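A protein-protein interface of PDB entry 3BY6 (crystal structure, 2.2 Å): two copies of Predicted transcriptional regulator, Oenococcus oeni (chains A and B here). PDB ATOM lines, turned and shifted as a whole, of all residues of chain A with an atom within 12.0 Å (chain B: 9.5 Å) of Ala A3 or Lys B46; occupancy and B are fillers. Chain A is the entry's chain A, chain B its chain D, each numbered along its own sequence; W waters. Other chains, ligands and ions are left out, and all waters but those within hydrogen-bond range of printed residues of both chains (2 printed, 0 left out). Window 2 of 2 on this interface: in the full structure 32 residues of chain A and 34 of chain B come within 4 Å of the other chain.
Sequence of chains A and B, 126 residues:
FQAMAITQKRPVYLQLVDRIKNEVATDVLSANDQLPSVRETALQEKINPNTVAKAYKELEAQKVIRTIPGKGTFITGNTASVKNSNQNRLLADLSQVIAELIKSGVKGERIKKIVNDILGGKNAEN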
ATOM      1  N   GLN A   2      23.239 -32.372  18.861  1.00  0.00           N
ATOM      2  CA  GLN A   2      22.784 -31.847  20.183  1.00  0.00           C
ATOM      3  C   GLN A   2      23.617 -30.669  20.726  1.00  0.00           C
ATOM      4  O   GLN A   2      23.196 -30.019  21.703  1.00  0.00           O
ATOM      5  CB  GLN A   2      22.813 -32.967  21.207  1.00  0.00           C
ATOM      6  CG  GLN A   2      21.744 -32.874  22.214  1.00  0.00           C
ATOM      7  CD  GLN A   2      22.178 -33.385  23.558  1.00  0.00           C
ATOM      8  OE1 GLN A   2      22.272 -32.610  24.545  1.00  0.00           O
ATOM      9  NE2 GLN A   2      22.441 -34.687  23.633  1.00  0.00           N
ATOM     10  N   ALA A   3      24.787 -30.399  20.128  1.00  0.00           N
ATOM     11  CA  ALA A   3      25.625 -29.280  20.558  1.00  0.00           C
ATOM     12  C   ALA A   3      24.838 -27.976  20.331  1.00  0.00           C
ATOM     13  O   ALA A   3      23.942 -27.929  19.486  1.00  0.00           O
ATOM     14  CB  ALA A   3      26.927 -29.266  19.819  1.00  0.00           C
ATOM     15  N   MET A   4      25.132 -26.939  21.109  1.00  0.00           N
ATOM     16  CA  MET A   4      24.329 -25.728  21.056  1.00  0.00           C
ATOM     17  C   MET A   4      24.548 -25.040  19.724  1.00  0.00           C
ATOM     18  O   MET A   4      25.632 -25.145  19.122  1.00  0.00           O
ATOM     19  CB  MET A   4      24.671 -24.769  22.197  1.00  0.00           C
ATOM     20  CG  MET A   4      26.069 -24.176  22.121  1.00  0.00           C
ATOM     21  SD  MET A   4      26.497 -23.100  23.498  1.00  0.00           S
ATOM     22  CE  MET A   4      25.571 -21.615  23.122  1.00  0.00           C
ATOM     23  N   ALA A   5      23.509 -24.334  19.279  1.00  0.00           N
ATOM     24  CA  ALA A   5      23.575 -23.510  18.071  1.00  0.00           C
ATOM     25  C   ALA A   5      24.235 -22.189  18.453  1.00  0.00           C
ATOM     26  O   ALA A   5      23.947 -21.630  19.499  1.00  0.00           O
ATOM     27  CB  ALA A   5      22.180 -23.286  17.519  1.00  0.00           C
ATOM     28  N   ILE A   6      25.160 -21.721  17.641  1.00  0.00           N
ATOM     29  CA  ILE A   6      25.820 -20.463  17.895  1.00  0.00           C
ATOM     30  C   ILE A   6      25.198 -19.432  16.947  1.00  0.00           C
ATOM     31  O   ILE A   6      25.044 -19.685  15.755  1.00  0.00           O
ATOM     32  CB  ILE A   6      27.343 -20.568  17.658  1.00  0.00           C
ATOM     33  CG1 ILE A   6      27.903 -21.840  18.313  1.00  0.00           C
ATOM     34  CG2 ILE A   6      28.076 -19.311  18.163  1.00  0.00           C
ATOM     35  CD1 ILE A   6      27.656 -21.956  19.795  1.00  0.00           C
ATOM     36  N   THR A   7      24.832 -18.272  17.481  1.00  0.00           N
ATOM     37  CA  THR A   7      24.277 -17.205  16.664  1.00  0.00           C
ATOM     38  C   THR A   7      25.439 -16.360  16.149  1.00  0.00           C
ATOM     39  O   THR A   7      26.324 -15.945  16.912  1.00  0.00           O
ATOM     40  CB  THR A   7      23.304 -16.366  17.463  1.00  0.00           C
ATOM     41  OG1 THR A   7      24.042 -15.497  18.327  1.00  0.00           O
ATOM     42  CG2 THR A   7      22.375 -17.268  18.323  1.00  0.00           C
ATOM     43  N   GLN A   8      25.448 -16.122  14.838  1.00  0.00           N
ATOM     44  CA  GLN A   8      26.519 -15.377  14.215  1.00  0.00           C
ATOM     45  C   GLN A   8      26.148 -13.894  14.160  1.00  0.00           C
ATOM     46  O   GLN A   8      25.000 -13.517  14.419  1.00  0.00           O
ATOM     47  CB  GLN A   8      26.791 -15.925  12.813  1.00  0.00           C
ATOM     48  CG  GLN A   8      26.983 -17.466  12.714  1.00  0.00           C
ATOM     49  CD  GLN A   8      28.174 -17.997  13.526  1.00  0.00           C
ATOM     50  OE1 GLN A   8      29.278 -17.420  13.524  1.00  0.00           O
ATOM     51  NE2 GLN A   8      27.950 -19.119  14.218  1.00  0.00           N
ATOM     52  N   VAL B  12      31.302 -16.313  21.856  1.00  0.00           N
ATOM     53  CA  VAL B  12      30.780 -17.628  22.134  1.00  0.00           C
ATOM     54  C   VAL B  12      30.718 -17.900  23.662  1.00  0.00           C
ATOM     55  O   VAL B  12      29.758 -18.532  24.160  1.00  0.00           O
ATOM     56  CB  VAL B  12      31.561 -18.736  21.379  1.00  0.00           C
ATOM     57  CG1 VAL B  12      30.994 -20.114  21.714  1.00  0.00           C
ATOM     58  CG2 VAL B  12      31.483 -18.491  19.850  1.00  0.00           C
ATOM     59  N   LEU B  16      27.446 -19.178  25.853  1.00  0.00           N
ATOM     60  CA  LEU B  16      27.432 -20.334  26.743  1.00  0.00           C
ATOM     61  C   LEU B  16      27.078 -19.940  28.182  1.00  0.00           C
ATOM     62  O   LEU B  16      26.365 -20.670  28.841  1.00  0.00           O
ATOM     63  CB  LEU B  16      28.778 -21.055  26.746  1.00  0.00           C
ATOM     64  CG  LEU B  16      28.887 -22.295  27.652  1.00  0.00           C
ATOM     65  CD1 LEU B  16      27.749 -23.292  27.432  1.00  0.00           C
ATOM     66  CD2 LEU B  16      30.257 -22.942  27.379  1.00  0.00           C
ATOM     67  N   ARG B  19      23.505 -19.672  28.045  1.00  0.00           N
ATOM     68  CA  ARG B  19      22.819 -20.966  27.917  1.00  0.00           C
ATOM     69  C   ARG B  19      22.705 -21.600  29.293  1.00  0.00           C
ATOM     70  O   ARG B  19      21.639 -22.103  29.681  1.00  0.00           O
ATOM     71  CB  ARG B  19      23.558 -21.923  26.970  1.00  0.00           C
ATOM     72  CG  ARG B  19      22.943 -23.306  26.888  1.00  0.00           C
ATOM     73  CD  ARG B  19      23.847 -24.240  26.049  1.00  0.00           C
ATOM     74  NE  ARG B  19      23.188 -25.465  25.573  1.00  0.00           N
ATOM     75  CZ  ARG B  19      22.244 -25.517  24.625  1.00  0.00           C
ATOM     76  NH1 ARG B  19      21.777 -24.406  24.053  1.00  0.00           N
ATOM     77  NH2 ARG B  19      21.736 -26.691  24.258  1.00  0.00           N
ATOM     78  N   GLU B  23      19.331 -22.601  31.789  1.00  0.00           N
ATOM     79  CA  GLU B  23      19.096 -23.958  32.279  1.00  0.00           C
ATOM     80  C   GLU B  23      18.877 -23.947  33.784  1.00  0.00           C
ATOM     81  O   GLU B  23      18.017 -24.663  34.295  1.00  0.00           O
ATOM     82  CB  GLU B  23      20.264 -24.877  31.926  1.00  0.00           C
ATOM     83  CG  GLU B  23      20.282 -25.194  30.443  1.00  0.00           C
ATOM     84  CD  GLU B  23      21.404 -26.115  30.026  1.00  0.00           C
ATOM     85  OE1 GLU B  23      22.359 -26.324  30.804  1.00  0.00           O
ATOM     86  OE2 GLU B  23      21.328 -26.616  28.890  1.00  0.00           O
ATOM     87  N   VAL B  38      35.549 -28.496  32.069  1.00  0.00           N
ATOM     88  CA  VAL B  38      35.740 -27.628  30.935  1.00  0.00           C
ATOM     89  C   VAL B  38      35.850 -28.464  29.646  1.00  0.00           C
ATOM     90  O   VAL B  38      35.263 -28.127  28.610  1.00  0.00           O
ATOM     91  CB  VAL B  38      37.003 -26.739  31.134  1.00  0.00           C
ATOM     92  CG1 VAL B  38      37.499 -26.158  29.811  1.00  0.00           C
ATOM     93  CG2 VAL B  38      36.705 -25.629  32.131  1.00  0.00           C
ATOM     94  N   ARG B  39      36.593 -29.560  29.739  1.00  0.00           N
ATOM     95  CA  ARG B  39      36.807 -30.481  28.629  1.00  0.00           C
ATOM     96  C   ARG B  39      35.522 -31.191  28.202  1.00  0.00           C
ATOM     97  O   ARG B  39      35.246 -31.314  27.024  1.00  0.00           O
ATOM     98  CB  ARG B  39      37.831 -31.503  29.081  1.00  0.00           C
ATOM     99  CG  ARG B  39      38.577 -32.234  28.013  1.00  0.00           C
ATOM    100  CD  ARG B  39      40.051 -32.289  28.439  1.00  0.00           C
ATOM    101  NE  ARG B  39      40.785 -33.429  27.896  1.00  0.00           N
ATOM    102  CZ  ARG B  39      42.117 -33.485  27.772  1.00  0.00           C
ATOM    103  NH1 ARG B  39      42.887 -32.450  28.141  1.00  0.00           N
ATOM    104  NH2 ARG B  39      42.685 -34.586  27.262  1.00  0.00           N
ATOM    105  N   GLU B  40      34.726 -31.640  29.160  1.00  0.00           N
ATOM    106  CA  GLU B  40      33.438 -32.258  28.850  1.00  0.00           C
ATOM    107  C   GLU B  40      32.389 -31.304  28.317  1.00  0.00           C
ATOM    108  O   GLU B  40      31.526 -31.704  27.530  1.00  0.00           O
ATOM    109  CB  GLU B  40      32.866 -32.914  30.068  1.00  0.00           C
ATOM    110  CG  GLU B  40      33.700 -34.058  30.486  1.00  0.00           C
ATOM    111  CD  GLU B  40      33.377 -34.509  31.874  1.00  0.00           C
ATOM    112  OE1 GLU B  40      33.443 -33.672  32.820  1.00  0.00           O
ATOM    113  OE2 GLU B  40      33.063 -35.711  31.999  1.00  0.00           O
ATOM    114  N   THR B  41      32.402 -30.065  28.795  1.00  0.00           N
ATOM    115  CA  THR B  41      31.506 -29.064  28.227  1.00  0.00           C
ATOM    116  C   THR B  41      31.956 -28.681  26.792  1.00  0.00           C
ATOM    117  O   THR B  41      31.135 -28.574  25.903  1.00  0.00           O
ATOM    118  CB  THR B  41      31.327 -27.867  29.188  1.00  0.00           C
ATOM    119  OG1 THR B  41      30.680 -28.350  30.378  1.00  0.00           O
ATOM    120  CG2 THR B  41      30.477 -26.736  28.545  1.00  0.00           C
ATOM    121  N   ALA B  42      33.258 -28.494  26.591  1.00  0.00           N
ATOM    122  CA  ALA B  42      33.819 -28.261  25.284  1.00  0.00           C
ATOM    123  C   ALA B  42      33.415 -29.360  24.251  1.00  0.00           C
ATOM    124  O   ALA B  42      33.114 -29.045  23.095  1.00  0.00           O
ATOM    125  CB  ALA B  42      35.332 -28.105  25.390  1.00  0.00           C
ATOM    126  N   LEU B  43      33.345 -30.614  24.685  1.00  0.00           N
ATOM    127  CA  LEU B  43      32.873 -31.716  23.851  1.00  0.00           C
ATOM    128  C   LEU B  43      31.349 -31.779  23.686  1.00  0.00           C
ATOM    129  O   LEU B  43      30.858 -32.173  22.640  1.00  0.00           O
ATOM    130  CB  LEU B  43      33.359 -33.053  24.434  1.00  0.00           C
ATOM    131  CG  LEU B  43      32.963 -34.352  23.733  1.00  0.00           C
ATOM    132  CD1 LEU B  43      33.480 -34.372  22.300  1.00  0.00           C
ATOM    133  CD2 LEU B  43      33.492 -35.531  24.529  1.00  0.00           C
ATOM    134  N   GLN B  44      30.602 -31.435  24.710  1.00  0.00           N
ATOM    135  CA  GLN B  44      29.142 -31.302  24.595  1.00  0.00           C
ATOM    136  C   GLN B  44      28.757 -30.180  23.628  1.00  0.00           C
ATOM    137  O   GLN B  44      27.933 -30.392  22.756  1.00  0.00           O
ATOM    138  CB  GLN B  44      28.538 -31.050  25.975  1.00  0.00           C
ATOM    139  CG  GLN B  44      27.050 -30.746  26.044  1.00  0.00           C
ATOM    140  CD  GLN B  44      26.178 -31.838  25.498  1.00  0.00           C
ATOM    141  OE1 GLN B  44      26.270 -32.987  25.915  1.00  0.00           O
ATOM    142  NE2 GLN B  44      25.305 -31.481  24.534  1.00  0.00           N
ATOM    143  N   GLU B  45      29.367 -29.005  23.753  1.00  0.00           N
ATOM    144  CA  GLU B  45      28.941 -27.825  22.971  1.00  0.00           C
ATOM    145  C   GLU B  45      29.801 -27.562  21.725  1.00  0.00           C
ATOM    146  O   GLU B  45      29.544 -26.611  20.978  1.00  0.00           O
ATOM    147  CB  GLU B  45      28.903 -26.565  23.852  1.00  0.00           C
ATOM    148  CG  GLU B  45      28.095 -26.711  25.142  1.00  0.00           C
ATOM    149  CD  GLU B  45      26.627 -27.035  24.900  1.00  0.00           C
ATOM    150  OE1 GLU B  45      26.204 -27.322  23.764  1.00  0.00           O
ATOM    151  OE2 GLU B  45      25.864 -27.004  25.863  1.00  0.00           O
ATOM    152  N   LYS B  46      30.809 -28.407  21.517  1.00  0.00           N
ATOM    153  CA  LYS B  46      31.704 -28.325  20.366  1.00  0.00           C
ATOM    154  C   LYS B  46      32.416 -26.968  20.286  1.00  0.00           C
ATOM    155  O   LYS B  46      32.520 -26.365  19.219  1.00  0.00           O
ATOM    156  CB  LYS B  46      30.944 -28.651  19.079  1.00  0.00           C
ATOM    157  CG  LYS B  46      30.331 -30.026  19.076  1.00  0.00           C
ATOM    158  CD  LYS B  46      29.725 -30.328  17.718  1.00  0.00           C
ATOM    159  CE  LYS B  46      29.645 -31.792  17.379  1.00  0.00           C
ATOM    160  NZ  LYS B  46      29.551 -31.904  15.878  1.00  0.00           N
ATOM    161  N   ILE B  47      32.898 -26.509  21.442  1.00  0.00           N
ATOM    162  CA  ILE B  47      33.605 -25.231  21.588  1.00  0.00           C
ATOM    163  C   ILE B  47      35.048 -25.492  22.003  1.00  0.00           C
ATOM    164  O   ILE B  47      35.370 -26.542  22.556  1.00  0.00           O
ATOM    165  CB  ILE B  47      33.004 -24.380  22.743  1.00  0.00           C
ATOM    166  CG1 ILE B  47      31.496 -24.218  22.622  1.00  0.00           C
ATOM    167  CG2 ILE B  47      33.626 -23.003  22.802  1.00  0.00           C
ATOM    168  CD1 ILE B  47      30.941 -23.516  23.836  1.00  0.00           C
ATOM    169  N   ASN B  48      35.899 -24.512  21.750  1.00  0.00           N
ATOM    170  CA  ASN B  48      37.264 -24.469  22.258  1.00  0.00           C
ATOM    171  C   ASN B  48      37.214 -24.591  23.806  1.00  0.00           C
ATOM    172  O   ASN B  48      36.413 -23.931  24.463  1.00  0.00           O
ATOM    173  CB  ASN B  48      37.912 -23.160  21.734  1.00  0.00           C
ATOM    174  CG  ASN B  48      39.357 -22.944  22.197  1.00  0.00           C
ATOM    175  OD1 ASN B  48      40.019 -23.850  22.726  1.00  0.00           O
ATOM    176  ND2 ASN B  48      39.859 -21.715  21.988  1.00  0.00           N
ATOM    177  N   PRO B  49      38.002 -25.515  24.390  1.00  0.00           N
ATOM    178  CA  PRO B  49      38.122 -25.547  25.850  1.00  0.00           C
ATOM    179  C   PRO B  49      38.376 -24.189  26.526  1.00  0.00           C
ATOM    180  O   PRO B  49      37.776 -23.918  27.553  1.00  0.00           O
ATOM    181  CB  PRO B  49      39.287 -26.520  26.080  1.00  0.00           C
ATOM    182  CG  PRO B  49      39.216 -27.452  24.925  1.00  0.00           C
ATOM    183  CD  PRO B  49      38.752 -26.619  23.752  1.00  0.00           C
ATOM    184  N   THR B  51      37.470 -21.228  25.583  1.00  0.00           N
ATOM    185  CA  THR B  51      36.232 -20.473  25.497  1.00  0.00           C
ATOM    186  C   THR B  51      35.315 -20.918  26.629  1.00  0.00           C
ATOM    187  O   THR B  51      34.758 -20.095  27.331  1.00  0.00           O
ATOM    188  CB  THR B  51      35.604 -20.690  24.090  1.00  0.00           C
ATOM    189  OG1 THR B  51      36.517 -20.194  23.111  1.00  0.00           O
ATOM    190  CG2 THR B  51      34.233 -19.998  23.916  1.00  0.00           C
ATOM    191  N   VAL B  52      35.194 -22.228  26.818  1.00  0.00           N
ATOM    192  CA  VAL B  52      34.401 -22.772  27.914  1.00  0.00           C
ATOM    193  C   VAL B  52      34.977 -22.327  29.278  1.00  0.00           C
ATOM    194  O   VAL B  52      34.225 -21.984  30.197  1.00  0.00           O
ATOM    195  CB  VAL B  52      34.330 -24.307  27.844  1.00  0.00           C
ATOM    196  CG1 VAL B  52      33.744 -24.897  29.169  1.00  0.00           C
ATOM    197  CG2 VAL B  52      33.513 -24.751  26.605  1.00  0.00           C
HETATM  198  O   HOH W   1      24.135 -28.838  24.022  1.00  0.00           O
HETATM  199  O   HOH W   2      28.404 -25.369  18.792  1.00  0.00           O
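OE1 of Gln A2 is in hydrogen-bond range of NE2 of Gln B44 (3.2 Å). The side-chain carboxylate of Glu B45 sits at hydrogen-bond distance from the backbone NH of Met A4 (2.9 Å).
O of Ile A6 is in hydrogen-bond range of NE2 of Gln A8. NE of Arg B19 is in salt-bridge range of OE2 of Glu B23 (3.97 Å). The guanidinium group (NE) of Arg B19 lies within salt-bridge range of the side-chain carboxylate (OE2) of Glu B45 (3.1 Å).
Gln B44 touches Ala A3. C of Ala A3 touches OE1 of Glu B45 (3.8 Å). CB of Ala A3 touches CG of Lys B46, 3.6 Å away. CB of Met A4 touches NH1 of Arg B19 (3.5 Å). Ile A6 touches Val B12.
Of chain B, only Gln B44 (3.3 Å), Glu B45 (3.8 Å) and Lys B46 (3.6 Å) come within 4 Å of Ala A3. Glu B45 touches two residues of chain A. Of the printed residues of chain B, Gln A2 touches Gln B44. Of the printed residues of chain A, Val B12 touches Ile A6 (3.9 Å). Of the printed residues of chain B, Met A4 touches Arg B19 and Glu B45. The nearest residue of chain B that does not touch Ala A3 is Arg B19 (5.2 Å). The nearest residue of chain A that does not touch Lys B46 is Met A4 (5.9 Å). The nearest printed residue of chain B that does not touch Gln A2 is Arg B19 (4.4 Å).
Hydrophobic or aromatic side chains of chain A that line the printed part of chain B: Ala A3, Met A4 and Ile A6. Of the 18 printed residues of chain B, 5 touch a printed residue of chain A. Printed residues of chain B that touch a printed residue of chain A: Val B12, Arg B19, Gln B44, Glu B45 and Lys B46. Hydrophobic or aromatic side chains of chain B that line the printed part of chain A: Val B12. Among the printed residues, no Asp or Glu carboxylate lies within 4 Å of a Lys or Arg side-chain nitrogen of the other chain.
No position is printed for both chains.
Water W1 lies within hydrogen-bond range of OE1 of Glu B45 (2.6 Å), O of Gln A2 (2.8 Å), NE2 of Gln B44 (2.9 Å) and NH2 of Arg B19 (3.2 Å). Water W2 lies within hydrogen-bond range of the backbone carbonyl oxygen of Glu B45 (2.8 Å) and the backbone carbonyl oxygen of Met A4 (2.8 Å).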
